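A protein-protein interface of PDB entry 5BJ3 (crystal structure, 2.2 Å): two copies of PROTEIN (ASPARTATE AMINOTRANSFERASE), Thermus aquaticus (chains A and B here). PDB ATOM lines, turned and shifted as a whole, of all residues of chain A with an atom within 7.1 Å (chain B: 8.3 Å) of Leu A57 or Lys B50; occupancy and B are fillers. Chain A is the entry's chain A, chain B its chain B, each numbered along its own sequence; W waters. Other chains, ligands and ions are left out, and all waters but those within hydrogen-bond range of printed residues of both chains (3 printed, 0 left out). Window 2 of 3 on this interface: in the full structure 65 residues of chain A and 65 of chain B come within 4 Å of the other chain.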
ATOM      1  N   LYS A  50     -26.249   3.599  19.842  1.00  0.00           N
ATOM      2  CA  LYS A  50     -26.901   3.741  18.545  1.00  0.00           C
ATOM      3  C   LYS A  50     -26.601   5.115  17.945  1.00  0.00           C
ATOM      4  O   LYS A  50     -26.395   5.243  16.741  1.00  0.00           O
ATOM      5  CB  LYS A  50     -28.405   3.551  18.678  1.00  0.00           C
ATOM      6  CG  LYS A  50     -28.817   2.125  18.954  1.00  0.00           C
ATOM      7  CD  LYS A  50     -30.323   2.007  18.951  1.00  0.00           C
ATOM      8  CE  LYS A  50     -30.759   0.565  18.866  1.00  0.00           C
ATOM      9  NZ  LYS A  50     -32.240   0.484  18.863  1.00  0.00           N
ATOM     10  N   GLU A  51     -26.558   6.131  18.804  1.00  0.00           N
ATOM     11  CA  GLU A  51     -26.263   7.496  18.383  1.00  0.00           C
ATOM     12  C   GLU A  51     -24.866   7.625  17.810  1.00  0.00           C
ATOM     13  O   GLU A  51     -24.670   8.279  16.787  1.00  0.00           O
ATOM     14  CB  GLU A  51     -26.403   8.464  19.558  1.00  0.00           C
ATOM     15  CG  GLU A  51     -27.704   9.217  19.566  1.00  0.00           C
ATOM     16  CD  GLU A  51     -27.990   9.873  18.232  1.00  0.00           C
ATOM     17  OE1 GLU A  51     -27.164  10.691  17.775  1.00  0.00           O
ATOM     18  OE2 GLU A  51     -29.041   9.555  17.636  1.00  0.00           O
ATOM     19  N   ALA A  52     -23.891   7.029  18.491  1.00  0.00           N
ATOM     20  CA  ALA A  52     -22.504   7.074  18.042  1.00  0.00           C
ATOM     21  C   ALA A  52     -22.380   6.453  16.657  1.00  0.00           C
ATOM     22  O   ALA A  52     -21.600   6.920  15.828  1.00  0.00           O
ATOM     23  CB  ALA A  52     -21.615   6.349  19.026  1.00  0.00           C
ATOM     24  N   ALA A  53     -23.160   5.403  16.413  1.00  0.00           N
ATOM     25  CA  ALA A  53     -23.165   4.719  15.124  1.00  0.00           C
ATOM     26  C   ALA A  53     -23.734   5.657  14.060  1.00  0.00           C
ATOM     27  O   ALA A  53     -23.194   5.754  12.962  1.00  0.00           O
ATOM     28  CB  ALA A  53     -23.993   3.448  15.203  1.00  0.00           C
ATOM     29  N   ARG A  54     -24.818   6.351  14.399  1.00  0.00           N
ATOM     30  CA  ARG A  54     -25.447   7.297  13.480  1.00  0.00           C
ATOM     31  C   ARG A  54     -24.496   8.442  13.134  1.00  0.00           C
ATOM     32  O   ARG A  54     -24.437   8.872  11.983  1.00  0.00           O
ATOM     33  CB  ARG A  54     -26.746   7.847  14.074  1.00  0.00           C
ATOM     34  CG  ARG A  54     -27.854   6.814  14.191  1.00  0.00           C
ATOM     35  CD  ARG A  54     -29.042   7.364  14.960  1.00  0.00           C
ATOM     36  NE  ARG A  54     -30.048   6.333  15.202  1.00  0.00           N
ATOM     37  CZ  ARG A  54     -30.563   6.046  16.392  1.00  0.00           C
ATOM     38  NH1 ARG A  54     -30.179   6.715  17.472  1.00  0.00           N
ATOM     39  NH2 ARG A  54     -31.471   5.081  16.506  1.00  0.00           N
ATOM     40  N   ARG A  55     -23.745   8.921  14.125  1.00  0.00           N
ATOM     41  CA  ARG A  55     -22.789  10.001  13.898  1.00  0.00           C
ATOM     42  C   ARG A  55     -21.651   9.536  12.999  1.00  0.00           C
ATOM     43  O   ARG A  55     -21.142  10.305  12.180  1.00  0.00           O
ATOM     44  CB  ARG A  55     -22.224  10.530  15.220  1.00  0.00           C
ATOM     45  CG  ARG A  55     -23.249  11.239  16.093  1.00  0.00           C
ATOM     46  CD  ARG A  55     -22.580  12.107  17.157  1.00  0.00           C
ATOM     47  NE  ARG A  55     -21.729  11.340  18.063  1.00  0.00           N
ATOM     48  CZ  ARG A  55     -22.149  10.770  19.189  1.00  0.00           C
ATOM     49  NH1 ARG A  55     -23.419  10.872  19.565  1.00  0.00           N
ATOM     50  NH2 ARG A  55     -21.293  10.092  19.943  1.00  0.00           N
ATOM     51  N   ALA A  56     -21.250   8.275  13.158  1.00  0.00           N
ATOM     52  CA  ALA A  56     -20.176   7.701  12.353  1.00  0.00           C
ATOM     53  C   ALA A  56     -20.595   7.664  10.885  1.00  0.00           C
ATOM     54  O   ALA A  56     -19.817   8.022   9.998  1.00  0.00           O
ATOM     55  CB  ALA A  56     -19.840   6.299  12.847  1.00  0.00           C
ATOM     56  N   LEU A  57     -21.827   7.227  10.639  1.00  0.00           N
ATOM     57  CA  LEU A  57     -22.370   7.160   9.282  1.00  0.00           C
ATOM     58  C   LEU A  57     -22.358   8.550   8.665  1.00  0.00           C
ATOM     59  O   LEU A  57     -21.877   8.741   7.552  1.00  0.00           O
ATOM     60  CB  LEU A  57     -23.808   6.639   9.305  1.00  0.00           C
ATOM     61  CG  LEU A  57     -24.048   5.166   9.627  1.00  0.00           C
ATOM     62  CD1 LEU A  57     -25.535   4.917   9.812  1.00  0.00           C
ATOM     63  CD2 LEU A  57     -23.498   4.305   8.509  1.00  0.00           C
ATOM     64  N   ALA A  58     -22.869   9.521   9.417  1.00  0.00           N
ATOM     65  CA  ALA A  58     -22.935  10.906   8.974  1.00  0.00           C
ATOM     66  C   ALA A  58     -21.559  11.503   8.695  1.00  0.00           C
ATOM     67  O   ALA A  58     -21.406  12.327   7.795  1.00  0.00           O
ATOM     68  CB  ALA A  58     -23.677  11.746  10.004  1.00  0.00           C
ATOM     69  N   GLN A  59     -20.556  11.084   9.463  1.00  0.00           N
ATOM     70  CA  GLN A  59     -19.200  11.588   9.283  1.00  0.00           C
ATOM     71  C   GLN A  59     -18.415  10.828   8.217  1.00  0.00           C
ATOM     72  O   GLN A  59     -17.264  11.160   7.933  1.00  0.00           O
ATOM     73  CB  GLN A  59     -18.444  11.563  10.608  1.00  0.00           C
ATOM     74  CG  GLN A  59     -19.045  12.466  11.667  1.00  0.00           C
ATOM     75  CD  GLN A  59     -18.285  12.407  12.976  1.00  0.00           C
ATOM     76  OE1 GLN A  59     -17.290  13.106  13.158  1.00  0.00           O
ATOM     77  NE2 GLN A  59     -18.747  11.565  13.894  1.00  0.00           N
ATOM     78  N   GLY A  60     -19.041   9.813   7.630  1.00  0.00           N
ATOM     79  CA  GLY A  60     -18.386   9.030   6.595  1.00  0.00           C
ATOM     80  C   GLY A  60     -17.291   8.086   7.067  1.00  0.00           C
ATOM     81  O   GLY A  60     -16.339   7.831   6.330  1.00  0.00           O
ATOM     82  N   LYS A  61     -17.418   7.576   8.290  1.00  0.00           N
ATOM     83  CA  LYS A  61     -16.450   6.639   8.860  1.00  0.00           C
ATOM     84  C   LYS A  61     -16.789   5.258   8.301  1.00  0.00           C
ATOM     85  O   LYS A  61     -17.197   4.363   9.037  1.00  0.00           O
ATOM     86  CB  LYS A  61     -16.587   6.605  10.387  1.00  0.00           C
ATOM     87  CG  LYS A  61     -16.487   7.953  11.086  1.00  0.00           C
ATOM     88  CD  LYS A  61     -15.054   8.419  11.198  1.00  0.00           C
ATOM     89  CE  LYS A  61     -14.934   9.655  12.081  1.00  0.00           C
ATOM     90  NZ  LYS A  61     -15.531   9.458  13.432  1.00  0.00           N
ATOM     91  N   THR A  62     -16.584   5.086   6.998  1.00  0.00           N
ATOM     92  CA  THR A  62     -16.923   3.838   6.320  1.00  0.00           C
ATOM     93  C   THR A  62     -15.787   3.169   5.545  1.00  0.00           C
ATOM     94  O   THR A  62     -16.037   2.304   4.704  1.00  0.00           O
ATOM     95  CB  THR A  62     -18.064   4.088   5.332  1.00  0.00           C
ATOM     96  OG1 THR A  62     -17.638   5.069   4.376  1.00  0.00           O
ATOM     97  CG2 THR A  62     -19.301   4.602   6.053  1.00  0.00           C
ATOM     98  N   ILE A 270     -18.025   1.156  11.574  1.00  0.00           N
ATOM     99  CA  ILE A 270     -19.137   1.811  12.266  1.00  0.00           C
ATOM    100  C   ILE A 270     -19.320   1.210  13.668  1.00  0.00           C
ATOM    101  O   ILE A 270     -19.523   1.941  14.639  1.00  0.00           O
ATOM    102  CB  ILE A 270     -20.475   1.697  11.472  1.00  0.00           C
ATOM    103  CG1 ILE A 270     -20.427   2.563  10.210  1.00  0.00           C
ATOM    104  CG2 ILE A 270     -21.655   2.135  12.331  1.00  0.00           C
ATOM    105  CD1 ILE A 270     -19.882   1.861   8.995  1.00  0.00           C
ATOM    106  N   PHE B  43     -15.115   7.664  -2.800  1.00  0.00           N
ATOM    107  CA  PHE B  43     -16.509   8.028  -2.579  1.00  0.00           C
ATOM    108  C   PHE B  43     -16.986   7.402  -1.280  1.00  0.00           C
ATOM    109  O   PHE B  43     -16.506   6.341  -0.884  1.00  0.00           O
ATOM    110  CB  PHE B  43     -17.395   7.502  -3.717  1.00  0.00           C
ATOM    111  CG  PHE B  43     -17.116   8.133  -5.051  1.00  0.00           C
ATOM    112  CD1 PHE B  43     -17.650   9.377  -5.372  1.00  0.00           C
ATOM    113  CD2 PHE B  43     -16.324   7.482  -5.991  1.00  0.00           C
ATOM    114  CE1 PHE B  43     -17.396   9.967  -6.609  1.00  0.00           C
ATOM    115  CE2 PHE B  43     -16.065   8.063  -7.228  1.00  0.00           C
ATOM    116  CZ  PHE B  43     -16.606   9.309  -7.538  1.00  0.00           C
ATOM    117  N   ASP B  44     -17.918   8.073  -0.613  1.00  0.00           N
ATOM    118  CA  ASP B  44     -18.497   7.565   0.629  1.00  0.00           C
ATOM    119  C   ASP B  44     -19.626   6.633   0.179  1.00  0.00           C
ATOM    120  O   ASP B  44     -20.047   6.689  -0.977  1.00  0.00           O
ATOM    121  CB  ASP B  44     -19.054   8.730   1.456  1.00  0.00           C
ATOM    122  CG  ASP B  44     -19.415   8.338   2.886  1.00  0.00           C
ATOM    123  OD1 ASP B  44     -19.137   7.198   3.317  1.00  0.00           O
ATOM    124  OD2 ASP B  44     -19.978   9.200   3.590  1.00  0.00           O
ATOM    125  N   THR B  45     -20.095   5.752   1.060  1.00  0.00           N
ATOM    126  CA  THR B  45     -21.171   4.840   0.679  1.00  0.00           C
ATOM    127  C   THR B  45     -22.458   5.630   0.438  1.00  0.00           C
ATOM    128  O   THR B  45     -22.746   6.593   1.151  1.00  0.00           O
ATOM    129  CB  THR B  45     -21.369   3.676   1.708  1.00  0.00           C
ATOM    130  OG1 THR B  45     -22.701   3.677   2.221  1.00  0.00           O
ATOM    131  CG2 THR B  45     -20.396   3.783   2.843  1.00  0.00           C
ATOM    132  N   PRO B  46     -23.204   5.276  -0.622  1.00  0.00           N
ATOM    133  CA  PRO B  46     -24.463   5.934  -0.998  1.00  0.00           C
ATOM    134  C   PRO B  46     -25.528   6.016   0.101  1.00  0.00           C
ATOM    135  O   PRO B  46     -25.738   5.073   0.863  1.00  0.00           O
ATOM    136  CB  PRO B  46     -24.930   5.117  -2.205  1.00  0.00           C
ATOM    137  CG  PRO B  46     -24.266   3.779  -2.017  1.00  0.00           C
ATOM    138  CD  PRO B  46     -22.902   4.171  -1.548  1.00  0.00           C
ATOM    139  N   GLU B  47     -26.190   7.172   0.167  1.00  0.00           N
ATOM    140  CA  GLU B  47     -27.232   7.451   1.151  1.00  0.00           C
ATOM    141  C   GLU B  47     -28.323   6.407   1.320  1.00  0.00           C
ATOM    142  O   GLU B  47     -28.798   6.204   2.431  1.00  0.00           O
ATOM    143  CB  GLU B  47     -27.883   8.807   0.875  1.00  0.00           C
ATOM    144  CG  GLU B  47     -27.087   9.999   1.366  1.00  0.00           C
ATOM    145  CD  GLU B  47     -26.843   9.973   2.867  1.00  0.00           C
ATOM    146  OE1 GLU B  47     -27.735   9.563   3.633  1.00  0.00           O
ATOM    147  OE2 GLU B  47     -25.742  10.374   3.281  1.00  0.00           O
ATOM    148  N   HIS B  48     -28.747   5.766   0.234  1.00  0.00           N
ATOM    149  CA  HIS B  48     -29.794   4.759   0.358  1.00  0.00           C
ATOM    150  C   HIS B  48     -29.349   3.582   1.223  1.00  0.00           C
ATOM    151  O   HIS B  48     -30.167   2.965   1.907  1.00  0.00           O
ATOM    152  CB  HIS B  48     -30.311   4.294  -1.011  1.00  0.00           C
ATOM    153  CG  HIS B  48     -29.300   3.574  -1.847  1.00  0.00           C
ATOM    154  ND1 HIS B  48     -29.424   2.244  -2.189  1.00  0.00           N
ATOM    155  CD2 HIS B  48     -28.170   4.010  -2.459  1.00  0.00           C
ATOM    156  CE1 HIS B  48     -28.422   1.892  -2.971  1.00  0.00           C
ATOM    157  NE2 HIS B  48     -27.646   2.944  -3.150  1.00  0.00           N
ATOM    158  N   VAL B  49     -28.047   3.296   1.214  1.00  0.00           N
ATOM    159  CA  VAL B  49     -27.499   2.214   2.026  1.00  0.00           C
ATOM    160  C   VAL B  49     -27.398   2.681   3.480  1.00  0.00           C
ATOM    161  O   VAL B  49     -27.731   1.937   4.398  1.00  0.00           O
ATOM    162  CB  VAL B  49     -26.117   1.746   1.503  1.00  0.00           C
ATOM    163  CG1 VAL B  49     -25.496   0.742   2.465  1.00  0.00           C
ATOM    164  CG2 VAL B  49     -26.270   1.115   0.127  1.00  0.00           C
ATOM    165  N   LYS B  50     -26.963   3.925   3.677  1.00  0.00           N
ATOM    166  CA  LYS B  50     -26.853   4.491   5.015  1.00  0.00           C
ATOM    167  C   LYS B  50     -28.220   4.527   5.691  1.00  0.00           C
ATOM    168  O   LYS B  50     -28.332   4.275   6.892  1.00  0.00           O
ATOM    169  CB  LYS B  50     -26.270   5.899   4.953  1.00  0.00           C
ATOM    170  CG  LYS B  50     -24.807   5.936   4.589  1.00  0.00           C
ATOM    171  CD  LYS B  50     -24.277   7.354   4.673  1.00  0.00           C
ATOM    172  CE  LYS B  50     -22.767   7.377   4.672  1.00  0.00           C
ATOM    173  NZ  LYS B  50     -22.279   8.771   4.767  1.00  0.00           N
ATOM    174  N   GLU B  51     -29.255   4.823   4.908  1.00  0.00           N
ATOM    175  CA  GLU B  51     -30.626   4.878   5.407  1.00  0.00           C
ATOM    176  C   GLU B  51     -31.106   3.531   5.910  1.00  0.00           C
ATOM    177  O   GLU B  51     -31.734   3.444   6.965  1.00  0.00           O
ATOM    178  CB  GLU B  51     -31.577   5.363   4.317  1.00  0.00           C
ATOM    179  CG  GLU B  51     -31.945   6.812   4.439  1.00  0.00           C
ATOM    180  CD  GLU B  51     -32.424   7.165   5.829  1.00  0.00           C
ATOM    181  OE1 GLU B  51     -33.413   6.560   6.298  1.00  0.00           O
ATOM    182  OE2 GLU B  51     -31.803   8.046   6.453  1.00  0.00           O
ATOM    183  N   ALA B  52     -30.837   2.487   5.132  1.00  0.00           N
ATOM    184  CA  ALA B  52     -31.234   1.134   5.501  1.00  0.00           C
ATOM    185  C   ALA B  52     -30.597   0.745   6.831  1.00  0.00           C
ATOM    186  O   ALA B  52     -31.215   0.055   7.643  1.00  0.00           O
ATOM    187  CB  ALA B  52     -30.833   0.159   4.418  1.00  0.00           C
ATOM    188  N   ALA B  53     -29.360   1.199   7.044  1.00  0.00           N
ATOM    189  CA  ALA B  53     -28.631   0.925   8.280  1.00  0.00           C
ATOM    190  C   ALA B  53     -29.320   1.639   9.440  1.00  0.00           C
ATOM    191  O   ALA B  53     -29.509   1.061  10.506  1.00  0.00           O
ATOM    192  CB  ALA B  53     -27.186   1.389   8.155  1.00  0.00           C
ATOM    193  N   ARG B  54     -29.711   2.894   9.213  1.00  0.00           N
ATOM    194  CA  ARG B  54     -30.397   3.685  10.230  1.00  0.00           C
ATOM    195  C   ARG B  54     -31.738   3.054  10.604  1.00  0.00           C
ATOM    196  O   ARG B  54     -32.109   3.033  11.775  1.00  0.00           O
ATOM    197  CB  ARG B  54     -30.604   5.120   9.751  1.00  0.00           C
ATOM    198  CG  ARG B  54     -29.317   5.914   9.624  1.00  0.00           C
ATOM    199  CD  ARG B  54     -29.558   7.263   8.962  1.00  0.00           C
ATOM    200  NE  ARG B  54     -28.304   7.966   8.708  1.00  0.00           N
ATOM    201  CZ  ARG B  54     -27.948   8.470   7.530  1.00  0.00           C
ATOM    202  NH1 ARG B  54     -28.749   8.355   6.479  1.00  0.00           N
ATOM    203  NH2 ARG B  54     -26.780   9.090   7.402  1.00  0.00           N
ATOM    204  N   ARG B  55     -32.454   2.533   9.608  1.00  0.00           N
ATOM    205  CA  ARG B  55     -33.741   1.888   9.862  1.00  0.00           C
ATOM    206  C   ARG B  55     -33.557   0.602  10.657  1.00  0.00           C
ATOM    207  O   ARG B  55     -34.388   0.269  11.494  1.00  0.00           O
ATOM    208  CB  ARG B  55     -34.478   1.589   8.554  1.00  0.00           C
ATOM    209  CG  ARG B  55     -34.928   2.827   7.793  1.00  0.00           C
ATOM    210  CD  ARG B  55     -35.994   2.500   6.752  1.00  0.00           C
ATOM    211  NE  ARG B  55     -35.539   1.541   5.747  1.00  0.00           N
ATOM    212  CZ  ARG B  55     -34.934   1.873   4.611  1.00  0.00           C
ATOM    213  NH1 ARG B  55     -34.702   3.147   4.319  1.00  0.00           N
ATOM    214  NH2 ARG B  55     -34.560   0.925   3.760  1.00  0.00           N
ATOM    215  N   ALA B  56     -32.466  -0.114  10.389  1.00  0.00           N
ATOM    216  CA  ALA B  56     -32.162  -1.360  11.085  1.00  0.00           C
ATOM    217  C   ALA B  56     -31.929  -1.078  12.565  1.00  0.00           C
ATOM    218  O   ALA B  56     -32.430  -1.799  13.425  1.00  0.00           O
ATOM    219  CB  ALA B  56     -30.937  -2.019  10.474  1.00  0.00           C
ATOM    220  N   LEU B  57     -31.165  -0.026  12.849  1.00  0.00           N
ATOM    221  CA  LEU B  57     -30.880   0.377  14.223  1.00  0.00           C
ATOM    222  C   LEU B  57     -32.186   0.694  14.938  1.00  0.00           C
ATOM    223  O   LEU B  57     -32.443   0.200  16.035  1.00  0.00           O
ATOM    224  CB  LEU B  57     -29.989   1.622  14.241  1.00  0.00           C
ATOM    225  CG  LEU B  57     -28.524   1.477  13.827  1.00  0.00           C
ATOM    226  CD1 LEU B  57     -27.884   2.851  13.711  1.00  0.00           C
ATOM    227  CD2 LEU B  57     -27.785   0.628  14.848  1.00  0.00           C
ATOM    228  N   ALA B 237     -18.677   1.264  -2.390  1.00  0.00           N
ATOM    229  CA  ALA B 237     -17.862   2.023  -1.441  1.00  0.00           C
ATOM    230  C   ALA B 237     -18.213   1.626  -0.004  1.00  0.00           C
ATOM    231  O   ALA B 237     -18.494   2.473   0.843  1.00  0.00           O
ATOM    232  CB  ALA B 237     -18.065   3.524  -1.651  1.00  0.00           C
ATOM    233  N   MET B 238     -18.194   0.318   0.249  1.00  0.00           N
ATOM    234  CA  MET B 238     -18.525  -0.230   1.559  1.00  0.00           C
ATOM    235  C   MET B 238     -17.401  -1.089   2.145  1.00  0.00           C
ATOM    236  O   MET B 238     -17.663  -2.091   2.810  1.00  0.00           O
ATOM    237  CB  MET B 238     -19.811  -1.058   1.460  1.00  0.00           C
ATOM    238  CG  MET B 238     -21.080  -0.242   1.247  1.00  0.00           C
ATOM    239  SD  MET B 238     -22.517  -1.291   0.961  1.00  0.00           S
ATOM    240  CE  MET B 238     -22.845  -1.901   2.600  1.00  0.00           C
ATOM    241  N   TRP B 241     -17.615  -1.632   5.904  1.00  0.00           N
ATOM    242  CA  TRP B 241     -18.803  -2.335   6.392  1.00  0.00           C
ATOM    243  C   TRP B 241     -18.533  -3.821   6.583  1.00  0.00           C
ATOM    244  O   TRP B 241     -19.252  -4.500   7.312  1.00  0.00           O
ATOM    245  CB  TRP B 241     -19.978  -2.145   5.438  1.00  0.00           C
ATOM    246  CG  TRP B 241     -20.487  -0.745   5.381  1.00  0.00           C
ATOM    247  CD1 TRP B 241     -19.866   0.331   4.814  1.00  0.00           C
ATOM    248  CD2 TRP B 241     -21.739  -0.267   5.882  1.00  0.00           C
ATOM    249  NE1 TRP B 241     -20.658   1.447   4.926  1.00  0.00           N
ATOM    250  CE2 TRP B 241     -21.814   1.110   5.579  1.00  0.00           C
ATOM    251  CE3 TRP B 241     -22.809  -0.870   6.561  1.00  0.00           C
ATOM    252  CZ2 TRP B 241     -22.917   1.896   5.920  1.00  0.00           C
ATOM    253  CZ3 TRP B 241     -23.908  -0.086   6.902  1.00  0.00           C
ATOM    254  CH2 TRP B 241     -23.951   1.283   6.582  1.00  0.00           C
ATOM    255  N   ILE B 270     -26.418  -5.236  11.270  1.00  0.00           N
ATOM    256  CA  ILE B 270     -26.777  -3.944  10.689  1.00  0.00           C
ATOM    257  C   ILE B 270     -26.233  -3.828   9.261  1.00  0.00           C
ATOM    258  O   ILE B 270     -26.938  -3.373   8.358  1.00  0.00           O
ATOM    259  CB  ILE B 270     -26.262  -2.748  11.548  1.00  0.00           C
ATOM    260  CG1 ILE B 270     -27.041  -2.651  12.862  1.00  0.00           C
ATOM    261  CG2 ILE B 270     -26.409  -1.433  10.790  1.00  0.00           C
ATOM    262  CD1 ILE B 270     -26.453  -3.456  13.993  1.00  0.00           C
ATOM    263  N   ALA B 274     -28.162  -3.394   5.563  1.00  0.00           N
ATOM    264  CA  ALA B 274     -27.790  -2.271   4.714  1.00  0.00           C
ATOM    265  C   ALA B 274     -27.438  -2.788   3.320  1.00  0.00           C
ATOM    266  O   ALA B 274     -27.808  -2.186   2.316  1.00  0.00           O
ATOM    267  CB  ALA B 274     -26.610  -1.523   5.312  1.00  0.00           C
ATOM    268  N   THR B 275     -26.725  -3.913   3.275  1.00  0.00           N
ATOM    269  CA  THR B 275     -26.326  -4.535   2.017  1.00  0.00           C
ATOM    270  C   THR B 275     -27.561  -5.009   1.241  1.00  0.00           C
ATOM    271  O   THR B 275     -27.587  -4.950   0.016  1.00  0.00           O
ATOM    272  CB  THR B 275     -25.366  -5.720   2.269  1.00  0.00           C
ATOM    273  OG1 THR B 275     -24.223  -5.249   2.988  1.00  0.00           O
ATOM    274  CG2 THR B 275     -24.902  -6.342   0.953  1.00  0.00           C
ATOM    275  N   GLU B 277     -30.341  -3.565   1.039  1.00  0.00           N
ATOM    276  CA  GLU B 277     -30.830  -2.377   0.342  1.00  0.00           C
ATOM    277  C   GLU B 277     -30.012  -2.090  -0.909  1.00  0.00           C
ATOM    278  O   GLU B 277     -30.554  -1.674  -1.931  1.00  0.00           O
ATOM    279  CB  GLU B 277     -30.785  -1.168   1.276  1.00  0.00           C
ATOM    280  CG  GLU B 277     -31.207   0.157   0.641  1.00  0.00           C
ATOM    281  CD  GLU B 277     -32.694   0.237   0.315  1.00  0.00           C
ATOM    282  OE1 GLU B 277     -33.464  -0.670   0.697  1.00  0.00           O
ATOM    283  OE2 GLU B 277     -33.093   1.230  -0.326  1.00  0.00           O
ATOM    284  N   ALA B 278     -28.700  -2.291  -0.823  1.00  0.00           N
ATOM    285  CA  ALA B 278     -27.823  -2.060  -1.963  1.00  0.00           C
ATOM    286  C   ALA B 278     -28.171  -3.013  -3.106  1.00  0.00           C
ATOM    287  O   ALA B 278     -28.069  -2.655  -4.277  1.00  0.00           O
ATOM    288  CB  ALA B 278     -26.369  -2.230  -1.557  1.00  0.00           C
HETATM  289  O   HOH W   1     -16.690   4.446   1.696  1.00  0.00           O
HETATM  290  O   HOH W   2     -26.668   9.397  10.319  1.00  0.00           O
HETATM  291  O   HOH W   3     -31.844   5.156  13.445  1.00  0.00           O
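The side-chain amino group (NZ) of Lys A50 lies within hydrogen-bond range of the backbone carbonyl oxygen (O) of Leu B57 (2.8 Å). NZ of Lys B50 lies within hydrogen-bond range of O of Leu A57, at 2.8 Å. OD1 of Asp B44 is in hydrogen-bond range of OG1 of Thr A62 (2.8 Å).
The side-chain carboxylate (OE2) of Glu A51 is in salt-bridge range of the guanidinium group (NH1) of Arg A54 (3.1 Å). The side-chain carboxylate (OD2) of Asp B44 is in salt-bridge range of the side-chain amino group (NZ) of Lys B50 (2.6 Å). The side-chain carboxylate (OE1) of Glu B47 lies within salt-bridge range of the guanidinium group (NH1) of Arg B54, at 3.3 Å. The side-chain carboxylate of Glu B51 lies within salt-bridge range of the guanidinium group of Arg B54 (3.1 Å).
Among the printed residues, merely in contact across the chains: Arg A54 with Leu B57 (3.99 Å), Leu A57 with Arg B54 (3.9 Å), Leu A57 with Trp B241 (3.6 Å), Gly A60 with Asp B44 (3.4 Å), Thr A62 with Thr B45 (3.4 Å), Thr A62 with Trp B241 (3.6 Å) and Ile A270 with Trp B241 (3.996 Å).
Leu A57 touches three residues of chain B. No residue of chain B comes within 4 Å of Ala A56. No residue of chain B comes within 4 Å of Ala A58. Printed residues of chain B within 4 Å of Arg A54: Leu B57 (3.99 Å). Printed residues of chain A within 4 Å of Leu B57: Lys A50 and Arg A54. Of the printed residues of chain A, Arg B54 touches Leu A57 (3.9 Å). Printed residues of chain A within 4 Å of Thr B45: Thr A62 (3.4 Å). Ala A53 touches none of the printed residues of chain B. The nearest residue of chain A that does not touch Lys B50 is Gly A60 (4.3 Å).
Hydrophobic or aromatic side chains of chain B that line the printed part of chain A: Leu B57 and Trp B241. Of the 14 printed residues of chain A, 6 touch a printed residue of chain B. Among the printed residues, no Asp or Glu carboxylate lies within 4 Å of a Lys or Arg side-chain nitrogen of the other chain.
Lys A50 touches Leu B57, and with the chains exchanged Leu A57 touches Lys B50. Arg A54 touches Leu B57, and with the chains exchanged Leu A57 touches Arg B54. Of the 10 pairs that touch across the chains among the printed residues, 4 have their exchanged pair printed and touching as well.
Water W2 bridges NE of Arg B54 (2.7 Å) and O of Arg A54 (2.8 Å). Water W3 bridges O of Arg B54 and NE of Arg A54. Water W1 lies within hydrogen-bond range of the backbone carbonyl oxygen (O) of Ala B237 (2.8 Å), the side-chain hydroxyl (OG1) of Thr A62 (2.9 Å) and the backbone carbonyl oxygen (O) of Phe B43 (3.2 Å).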
